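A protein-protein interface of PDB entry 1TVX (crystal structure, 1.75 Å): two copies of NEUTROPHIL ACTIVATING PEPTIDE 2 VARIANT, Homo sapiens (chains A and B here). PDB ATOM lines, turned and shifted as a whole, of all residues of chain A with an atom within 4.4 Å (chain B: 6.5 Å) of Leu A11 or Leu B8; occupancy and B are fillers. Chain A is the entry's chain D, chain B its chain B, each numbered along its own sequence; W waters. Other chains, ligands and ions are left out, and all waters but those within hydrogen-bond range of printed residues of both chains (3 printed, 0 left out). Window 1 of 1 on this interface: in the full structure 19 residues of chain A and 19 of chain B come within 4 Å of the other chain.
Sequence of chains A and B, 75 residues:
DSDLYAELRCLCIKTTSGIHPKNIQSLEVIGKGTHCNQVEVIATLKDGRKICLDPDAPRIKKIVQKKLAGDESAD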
ATOM      1  N   LEU A   8     -29.124   8.389 -14.359  1.00  0.00           N
ATOM      2  CA  LEU A   8     -29.071   9.625 -13.616  1.00  0.00           C
ATOM      3  C   LEU A   8     -30.146  10.537 -14.232  1.00  0.00           C
ATOM      4  O   LEU A   8     -30.103  10.868 -15.414  1.00  0.00           O
ATOM      5  CB  LEU A   8     -27.686  10.291 -13.799  1.00  0.00           C
ATOM      6  CG  LEU A   8     -27.477  11.657 -13.104  1.00  0.00           C
ATOM      7  CD1 LEU A   8     -27.518  11.500 -11.591  1.00  0.00           C
ATOM      8  CD2 LEU A   8     -26.135  12.254 -13.571  1.00  0.00           C
ATOM      9  N   ARG A   9     -31.099  10.962 -13.415  1.00  0.00           N
ATOM     10  CA  ARG A   9     -32.162  11.835 -13.905  1.00  0.00           C
ATOM     11  C   ARG A   9     -32.048  13.245 -13.258  1.00  0.00           C
ATOM     12  O   ARG A   9     -30.983  13.878 -13.361  1.00  0.00           O
ATOM     13  CB  ARG A   9     -33.540  11.141 -13.727  1.00  0.00           C
ATOM     14  CG  ARG A   9     -33.654   9.781 -14.511  1.00  0.00           C
ATOM     15  CD  ARG A   9     -35.077   9.256 -14.617  1.00  0.00           C
ATOM     16  NE  ARG A   9     -35.985  10.296 -15.101  1.00  0.00           N
ATOM     17  CZ  ARG A   9     -36.116  10.680 -16.370  1.00  0.00           C
ATOM     18  NH1 ARG A   9     -35.429  10.081 -17.342  1.00  0.00           N
ATOM     19  NH2 ARG A   9     -36.958  11.652 -16.671  1.00  0.00           N
ATOM     20  N   CYS A  10     -33.098  13.738 -12.583  1.00  0.00           N
ATOM     21  CA  CYS A  10     -33.004  15.083 -11.978  1.00  0.00           C
ATOM     22  C   CYS A  10     -31.985  15.146 -10.873  1.00  0.00           C
ATOM     23  O   CYS A  10     -31.888  14.252 -10.032  1.00  0.00           O
ATOM     24  CB  CYS A  10     -34.366  15.610 -11.484  1.00  0.00           C
ATOM     25  SG  CYS A  10     -35.618  15.666 -12.807  1.00  0.00           S
ATOM     26  N   LEU A  11     -31.269  16.242 -10.864  1.00  0.00           N
ATOM     27  CA  LEU A  11     -30.202  16.495  -9.900  1.00  0.00           C
ATOM     28  C   LEU A  11     -30.613  17.335  -8.691  1.00  0.00           C
ATOM     29  O   LEU A  11     -30.074  17.160  -7.602  1.00  0.00           O
ATOM     30  CB  LEU A  11     -29.089  17.256 -10.614  1.00  0.00           C
ATOM     31  CG  LEU A  11     -28.013  16.546 -11.412  1.00  0.00           C
ATOM     32  CD1 LEU A  11     -28.323  15.094 -11.753  1.00  0.00           C
ATOM     33  CD2 LEU A  11     -27.700  17.405 -12.580  1.00  0.00           C
ATOM     34  N   CYS A  12     -31.574  18.231  -8.886  1.00  0.00           N
ATOM     35  CA  CYS A  12     -31.957  19.178  -7.835  1.00  0.00           C
ATOM     36  C   CYS A  12     -33.368  19.080  -7.345  1.00  0.00           C
ATOM     37  O   CYS A  12     -34.266  19.680  -7.946  1.00  0.00           O
ATOM     38  CB  CYS A  12     -31.793  20.595  -8.384  1.00  0.00           C
ATOM     39  SG  CYS A  12     -30.094  21.031  -8.790  1.00  0.00           S
ATOM     40  N   ILE A  13     -33.610  18.342  -6.290  1.00  0.00           N
ATOM     41  CA  ILE A  13     -34.995  18.339  -5.839  1.00  0.00           C
ATOM     42  C   ILE A  13     -35.159  19.515  -4.852  1.00  0.00           C
ATOM     43  O   ILE A  13     -36.172  20.210  -4.891  1.00  0.00           O
ATOM     44  CB  ILE A  13     -35.513  16.932  -5.431  1.00  0.00           C
ATOM     45  CG1 ILE A  13     -35.529  16.016  -6.677  1.00  0.00           C
ATOM     46  CG2 ILE A  13     -36.956  17.012  -4.956  1.00  0.00           C
ATOM     47  CD1 ILE A  13     -36.384  16.530  -7.860  1.00  0.00           C
ATOM     48  N   GLU A  40     -33.165  22.803 -14.549  1.00  0.00           N
ATOM     49  CA  GLU A  40     -32.264  22.801 -13.397  1.00  0.00           C
ATOM     50  C   GLU A  40     -31.146  23.786 -13.624  1.00  0.00           C
ATOM     51  O   GLU A  40     -30.706  23.944 -14.745  1.00  0.00           O
ATOM     52  CB  GLU A  40     -31.760  21.378 -13.071  1.00  0.00           C
ATOM     53  CG  GLU A  40     -32.909  20.427 -12.817  1.00  0.00           C
ATOM     54  CD  GLU A  40     -32.527  19.175 -12.062  1.00  0.00           C
ATOM     55  OE1 GLU A  40     -31.652  18.419 -12.522  1.00  0.00           O
ATOM     56  OE2 GLU A  40     -33.161  18.915 -11.029  1.00  0.00           O
ATOM     57  N   ILE A  42     -27.457  24.970 -11.917  1.00  0.00           N
ATOM     58  CA  ILE A  42     -26.424  24.606 -10.926  1.00  0.00           C
ATOM     59  C   ILE A  42     -25.364  25.700 -10.944  1.00  0.00           C
ATOM     60  O   ILE A  42     -24.845  26.049 -12.029  1.00  0.00           O
ATOM     61  CB  ILE A  42     -25.707  23.255 -11.273  1.00  0.00           C
ATOM     62  CG1 ILE A  42     -26.694  22.189 -11.844  1.00  0.00           C
ATOM     63  CG2 ILE A  42     -24.941  22.749 -10.037  1.00  0.00           C
ATOM     64  CD1 ILE A  42     -27.486  21.481 -10.826  1.00  0.00           C
ATOM     65  N   LYS A  50     -21.037  23.108  -5.369  1.00  0.00           N
ATOM     66  CA  LYS A  50     -22.122  23.403  -6.296  1.00  0.00           C
ATOM     67  C   LYS A  50     -23.476  23.531  -5.631  1.00  0.00           C
ATOM     68  O   LYS A  50     -23.793  22.771  -4.701  1.00  0.00           O
ATOM     69  CB  LYS A  50     -22.204  22.270  -7.328  1.00  0.00           C
ATOM     70  CG  LYS A  50     -20.993  22.165  -8.258  1.00  0.00           C
ATOM     71  CD  LYS A  50     -21.135  20.939  -9.107  1.00  0.00           C
ATOM     72  CE  LYS A  50     -20.046  20.824 -10.122  1.00  0.00           C
ATOM     73  NZ  LYS A  50     -18.812  20.327  -9.527  1.00  0.00           N
ATOM     74  N   CYS A  52     -27.835  24.076  -6.158  1.00  0.00           N
ATOM     75  CA  CYS A  52     -29.089  24.056  -6.937  1.00  0.00           C
ATOM     76  C   CYS A  52     -29.898  25.337  -6.753  1.00  0.00           C
ATOM     77  O   CYS A  52     -30.450  25.570  -5.663  1.00  0.00           O
ATOM     78  CB  CYS A  52     -29.939  22.895  -6.455  1.00  0.00           C
ATOM     79  SG  CYS A  52     -29.278  21.273  -6.960  1.00  0.00           S
ATOM     80  N   ASP B   3     -22.850  20.320   4.823  1.00  0.00           N
ATOM     81  CA  ASP B   3     -23.490  20.804   3.615  1.00  0.00           C
ATOM     82  C   ASP B   3     -24.011  22.225   3.680  1.00  0.00           C
ATOM     83  O   ASP B   3     -24.557  22.660   4.701  1.00  0.00           O
ATOM     84  CB  ASP B   3     -24.714  19.966   3.319  1.00  0.00           C
ATOM     85  CG  ASP B   3     -24.406  18.733   2.561  1.00  0.00           C
ATOM     86  OD1 ASP B   3     -23.330  18.140   2.830  1.00  0.00           O
ATOM     87  OD2 ASP B   3     -25.262  18.358   1.710  1.00  0.00           O
ATOM     88  N   LEU B   4     -23.850  22.940   2.576  1.00  0.00           N
ATOM     89  CA  LEU B   4     -24.423  24.258   2.450  1.00  0.00           C
ATOM     90  C   LEU B   4     -25.874  23.936   2.006  1.00  0.00           C
ATOM     91  O   LEU B   4     -26.179  22.821   1.510  1.00  0.00           O
ATOM     92  CB  LEU B   4     -23.682  25.089   1.399  1.00  0.00           C
ATOM     93  CG  LEU B   4     -22.206  25.365   1.701  1.00  0.00           C
ATOM     94  CD1 LEU B   4     -21.576  25.989   0.504  1.00  0.00           C
ATOM     95  CD2 LEU B   4     -22.051  26.288   2.918  1.00  0.00           C
ATOM     96  N   ALA B   6     -29.047  23.411  -0.070  1.00  0.00           N
ATOM     97  CA  ALA B   6     -29.273  23.098  -1.485  1.00  0.00           C
ATOM     98  C   ALA B   6     -28.011  22.685  -2.278  1.00  0.00           C
ATOM     99  O   ALA B   6     -28.001  22.704  -3.521  1.00  0.00           O
ATOM    100  CB  ALA B   6     -29.967  24.255  -2.169  1.00  0.00           C
ATOM    101  N   GLU B   7     -26.977  22.253  -1.560  1.00  0.00           N
ATOM    102  CA  GLU B   7     -25.727  21.826  -2.181  1.00  0.00           C
ATOM    103  C   GLU B   7     -25.894  20.501  -2.941  1.00  0.00           C
ATOM    104  O   GLU B   7     -26.604  19.576  -2.480  1.00  0.00           O
ATOM    105  CB  GLU B   7     -24.634  21.673  -1.120  1.00  0.00           C
ATOM    106  CG  GLU B   7     -23.255  21.254  -1.681  1.00  0.00           C
ATOM    107  CD  GLU B   7     -22.141  21.210  -0.615  1.00  0.00           C
ATOM    108  OE1 GLU B   7     -22.423  21.287   0.600  1.00  0.00           O
ATOM    109  OE2 GLU B   7     -20.960  21.089  -1.014  1.00  0.00           O
ATOM    110  N   LEU B   8     -25.211  20.417  -4.080  1.00  0.00           N
ATOM    111  CA  LEU B   8     -25.206  19.234  -4.914  1.00  0.00           C
ATOM    112  C   LEU B   8     -23.813  18.627  -4.807  1.00  0.00           C
ATOM    113  O   LEU B   8     -22.834  19.278  -5.180  1.00  0.00           O
ATOM    114  CB  LEU B   8     -25.460  19.644  -6.372  1.00  0.00           C
ATOM    115  CG  LEU B   8     -25.356  18.527  -7.417  1.00  0.00           C
ATOM    116  CD1 LEU B   8     -26.361  17.428  -7.179  1.00  0.00           C
ATOM    117  CD2 LEU B   8     -25.529  19.130  -8.788  1.00  0.00           C
ATOM    118  N   ARG B   9     -23.729  17.392  -4.301  1.00  0.00           N
ATOM    119  CA  ARG B   9     -22.446  16.675  -4.157  1.00  0.00           C
ATOM    120  C   ARG B   9     -22.292  15.534  -5.179  1.00  0.00           C
ATOM    121  O   ARG B   9     -22.482  15.749  -6.381  1.00  0.00           O
ATOM    122  CB  ARG B   9     -22.287  16.133  -2.755  1.00  0.00           C
ATOM    123  CG  ARG B   9     -22.453  17.186  -1.732  1.00  0.00           C
ATOM    124  CD  ARG B   9     -21.692  16.857  -0.513  1.00  0.00           C
ATOM    125  NE  ARG B   9     -20.659  17.842  -0.473  1.00  0.00           N
ATOM    126  CZ  ARG B   9     -19.372  17.584  -0.600  1.00  0.00           C
ATOM    127  NH1 ARG B   9     -18.921  16.342  -0.648  1.00  0.00           N
ATOM    128  NH2 ARG B   9     -18.543  18.598  -0.597  1.00  0.00           N
ATOM    129  N   CYS B  10     -21.970  14.325  -4.716  1.00  0.00           N
ATOM    130  CA  CYS B  10     -21.820  13.207  -5.661  1.00  0.00           C
ATOM    131  C   CYS B  10     -23.132  12.871  -6.340  1.00  0.00           C
ATOM    132  O   CYS B  10     -24.170  12.786  -5.705  1.00  0.00           O
ATOM    133  CB  CYS B  10     -21.280  11.946  -4.975  1.00  0.00           C
ATOM    134  SG  CYS B  10     -19.691  12.237  -4.176  1.00  0.00           S
ATOM    135  N   LEU B  11     -23.028  12.565  -7.617  1.00  0.00           N
ATOM    136  CA  LEU B  11     -24.150  12.270  -8.488  1.00  0.00           C
ATOM    137  C   LEU B  11     -24.448  10.789  -8.671  1.00  0.00           C
ATOM    138  O   LEU B  11     -25.601  10.409  -8.894  1.00  0.00           O
ATOM    139  CB  LEU B  11     -23.816  12.878  -9.874  1.00  0.00           C
ATOM    140  CG  LEU B  11     -23.914  14.383 -10.242  1.00  0.00           C
ATOM    141  CD1 LEU B  11     -23.439  15.296  -9.185  1.00  0.00           C
ATOM    142  CD2 LEU B  11     -23.194  14.637 -11.525  1.00  0.00           C
ATOM    143  N   HIS B  35     -16.510  19.088  -4.104  1.00  0.00           N
ATOM    144  CA  HIS B  35     -17.928  18.799  -4.334  1.00  0.00           C
ATOM    145  C   HIS B  35     -18.255  17.329  -4.140  1.00  0.00           C
ATOM    146  O   HIS B  35     -19.392  16.963  -3.901  1.00  0.00           O
ATOM    147  CB  HIS B  35     -18.258  19.143  -5.795  1.00  0.00           C
ATOM    148  CG  HIS B  35     -17.423  18.387  -6.799  1.00  0.00           C
ATOM    149  ND1 HIS B  35     -16.080  18.646  -7.008  1.00  0.00           N
ATOM    150  CD2 HIS B  35     -17.742  17.381  -7.644  1.00  0.00           C
ATOM    151  CE1 HIS B  35     -15.612  17.829  -7.936  1.00  0.00           C
ATOM    152  NE2 HIS B  35     -16.601  17.051  -8.337  1.00  0.00           N
ATOM    153  N   CYS B  36     -17.248  16.477  -4.310  1.00  0.00           N
ATOM    154  CA  CYS B  36     -17.420  15.005  -4.254  1.00  0.00           C
ATOM    155  C   CYS B  36     -16.050  14.316  -4.267  1.00  0.00           C
ATOM    156  O   CYS B  36     -15.249  14.508  -5.193  1.00  0.00           O
ATOM    157  CB  CYS B  36     -18.219  14.546  -5.470  1.00  0.00           C
ATOM    158  SG  CYS B  36     -18.425  12.739  -5.643  1.00  0.00           S
ATOM    159  N   LYS B  50     -28.993   9.728 -19.365  1.00  0.00           N
ATOM    160  CA  LYS B  50     -27.630   9.704 -18.818  1.00  0.00           C
ATOM    161  C   LYS B  50     -27.415   8.539 -17.921  1.00  0.00           C
ATOM    162  O   LYS B  50     -28.344   8.114 -17.219  1.00  0.00           O
ATOM    163  CB  LYS B  50     -27.353  10.990 -18.012  1.00  0.00           C
ATOM    164  CG  LYS B  50     -27.467  12.203 -18.860  1.00  0.00           C
ATOM    165  CD  LYS B  50     -27.263  13.456 -18.132  1.00  0.00           C
ATOM    166  CE  LYS B  50     -27.353  14.547 -19.142  1.00  0.00           C
ATOM    167  NZ  LYS B  50     -28.186  15.640 -18.650  1.00  0.00           N
HETATM  168  O   HOH W   1     -20.732  20.621  -3.949  1.00  0.00           O
HETATM  169  O   HOH W   2     -31.413  10.142 -17.761  1.00  0.00           O
HETATM  170  O   HOH W   3     -30.298  20.273  -3.855  1.00  0.00           O
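Among the printed residues, merely in contact across the chains: Lys A50 with Glu B7 (3.3 Å), Leu A8 with Leu B11 (3.5 Å), Lys A50 with His B35 (3.6 Å), Ile A42 with Leu B8 (3.7 Å) and Leu A11 with Leu B8 (3.7 Å).
Of the 11 printed residues of chain B, 6 touch a printed residue of chain A.
Printed residues of chain A that touch a printed residue of chain B: Leu A8, Leu A11, Ile A42, Lys A50 and Cys A52.
Hydrophobic or aromatic side chains of chain A that line the printed part of chain B: Leu A8 and Ile A42.
Among the printed residues, 8 pairs touch across the chains.
Among the printed residues, no Asp or Glu carboxylate lies within 4 Å of a Lys or Arg side-chain nitrogen of the other chain.
Water W1 lies within hydrogen-bond range of O of Leu B8, N of Lys A50 and OE2 of Glu B7.
Water W2 bridges the backbone carbonyl oxygen (O) of Leu A8 (2.8 Å) and the backbone NH (N) of Lys B50 (2.9 Å).
Water W3 bridges O of Ala B6 and SG of Cys A52.
Leu A11 touches one residue of chain B.
Of chain A, only Leu A11, Ile A42 and Lys A50 come within 4 Å of Leu B8.
Of the printed residues of chain B, Leu A8 touches Leu B11 and Lys B50.
Of the printed residues of chain B, Ile A42 touches Leu B8.
Of the printed residues of chain A, Lys B50 touches Leu A8 (3.0 Å).
Printed residues of chain A within 4 Å of His B35: Lys A50 (3.6 Å).
Of the printed residues of chain A, Ala B6 touches Cys A52.
The nearest residue of chain A that does not touch Leu B8 is Cys A52 (4.2 Å).
The nearest printed residue of chain A that does not touch Leu B11 is Leu A11 (4.7 Å).
Leu A8 touches Leu B11, and with the chains exchanged Leu A11 touches Leu B8.
Leu A8 touches Lys B50, and with the chains exchanged Lys A50 touches Leu B8.
Positions printed for both chains: 8, 9, 10, 11 and 50.
Of the 8 pairs that touch across the chains among the printed residues, 4 have their exchanged pair printed and touching as well.
N of Leu B4 sits at hydrogen-bond distance from OE1 of Glu B7.
The side-chain carboxylate of Glu B7 is in salt-bridge range of the guanidinium group of Arg B9, at 3.3 Å.
The backbone carbonyl oxygen (O) of His B35 sits close to the guanidinium group (NH1) of Arg B9 (3.3 Å).
OE1 of Glu A40 is in hydrogen-bond range of N of Leu A11 (2.8 Å).
The side-chain sulfur (SG) of Cys A12 is disulfide-bonded to the side-chain sulfur (SG) of Cys A52 (2.0 Å).
The side-chain sulfur (SG) of Cys B10 forms a disulfide with the side-chain sulfur (SG) of Cys B36 (2.0 Å).
O of Ala B6 is in hydrogen-bond range of N of Cys A52, at 3.0 Å.
The backbone NH (N) of Leu B8 sits at hydrogen-bond distance from the backbone carbonyl oxygen (O) of Lys A50.
O of Lys B50 is in hydrogen-bond range of N of Leu A8 (3.0 Å).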
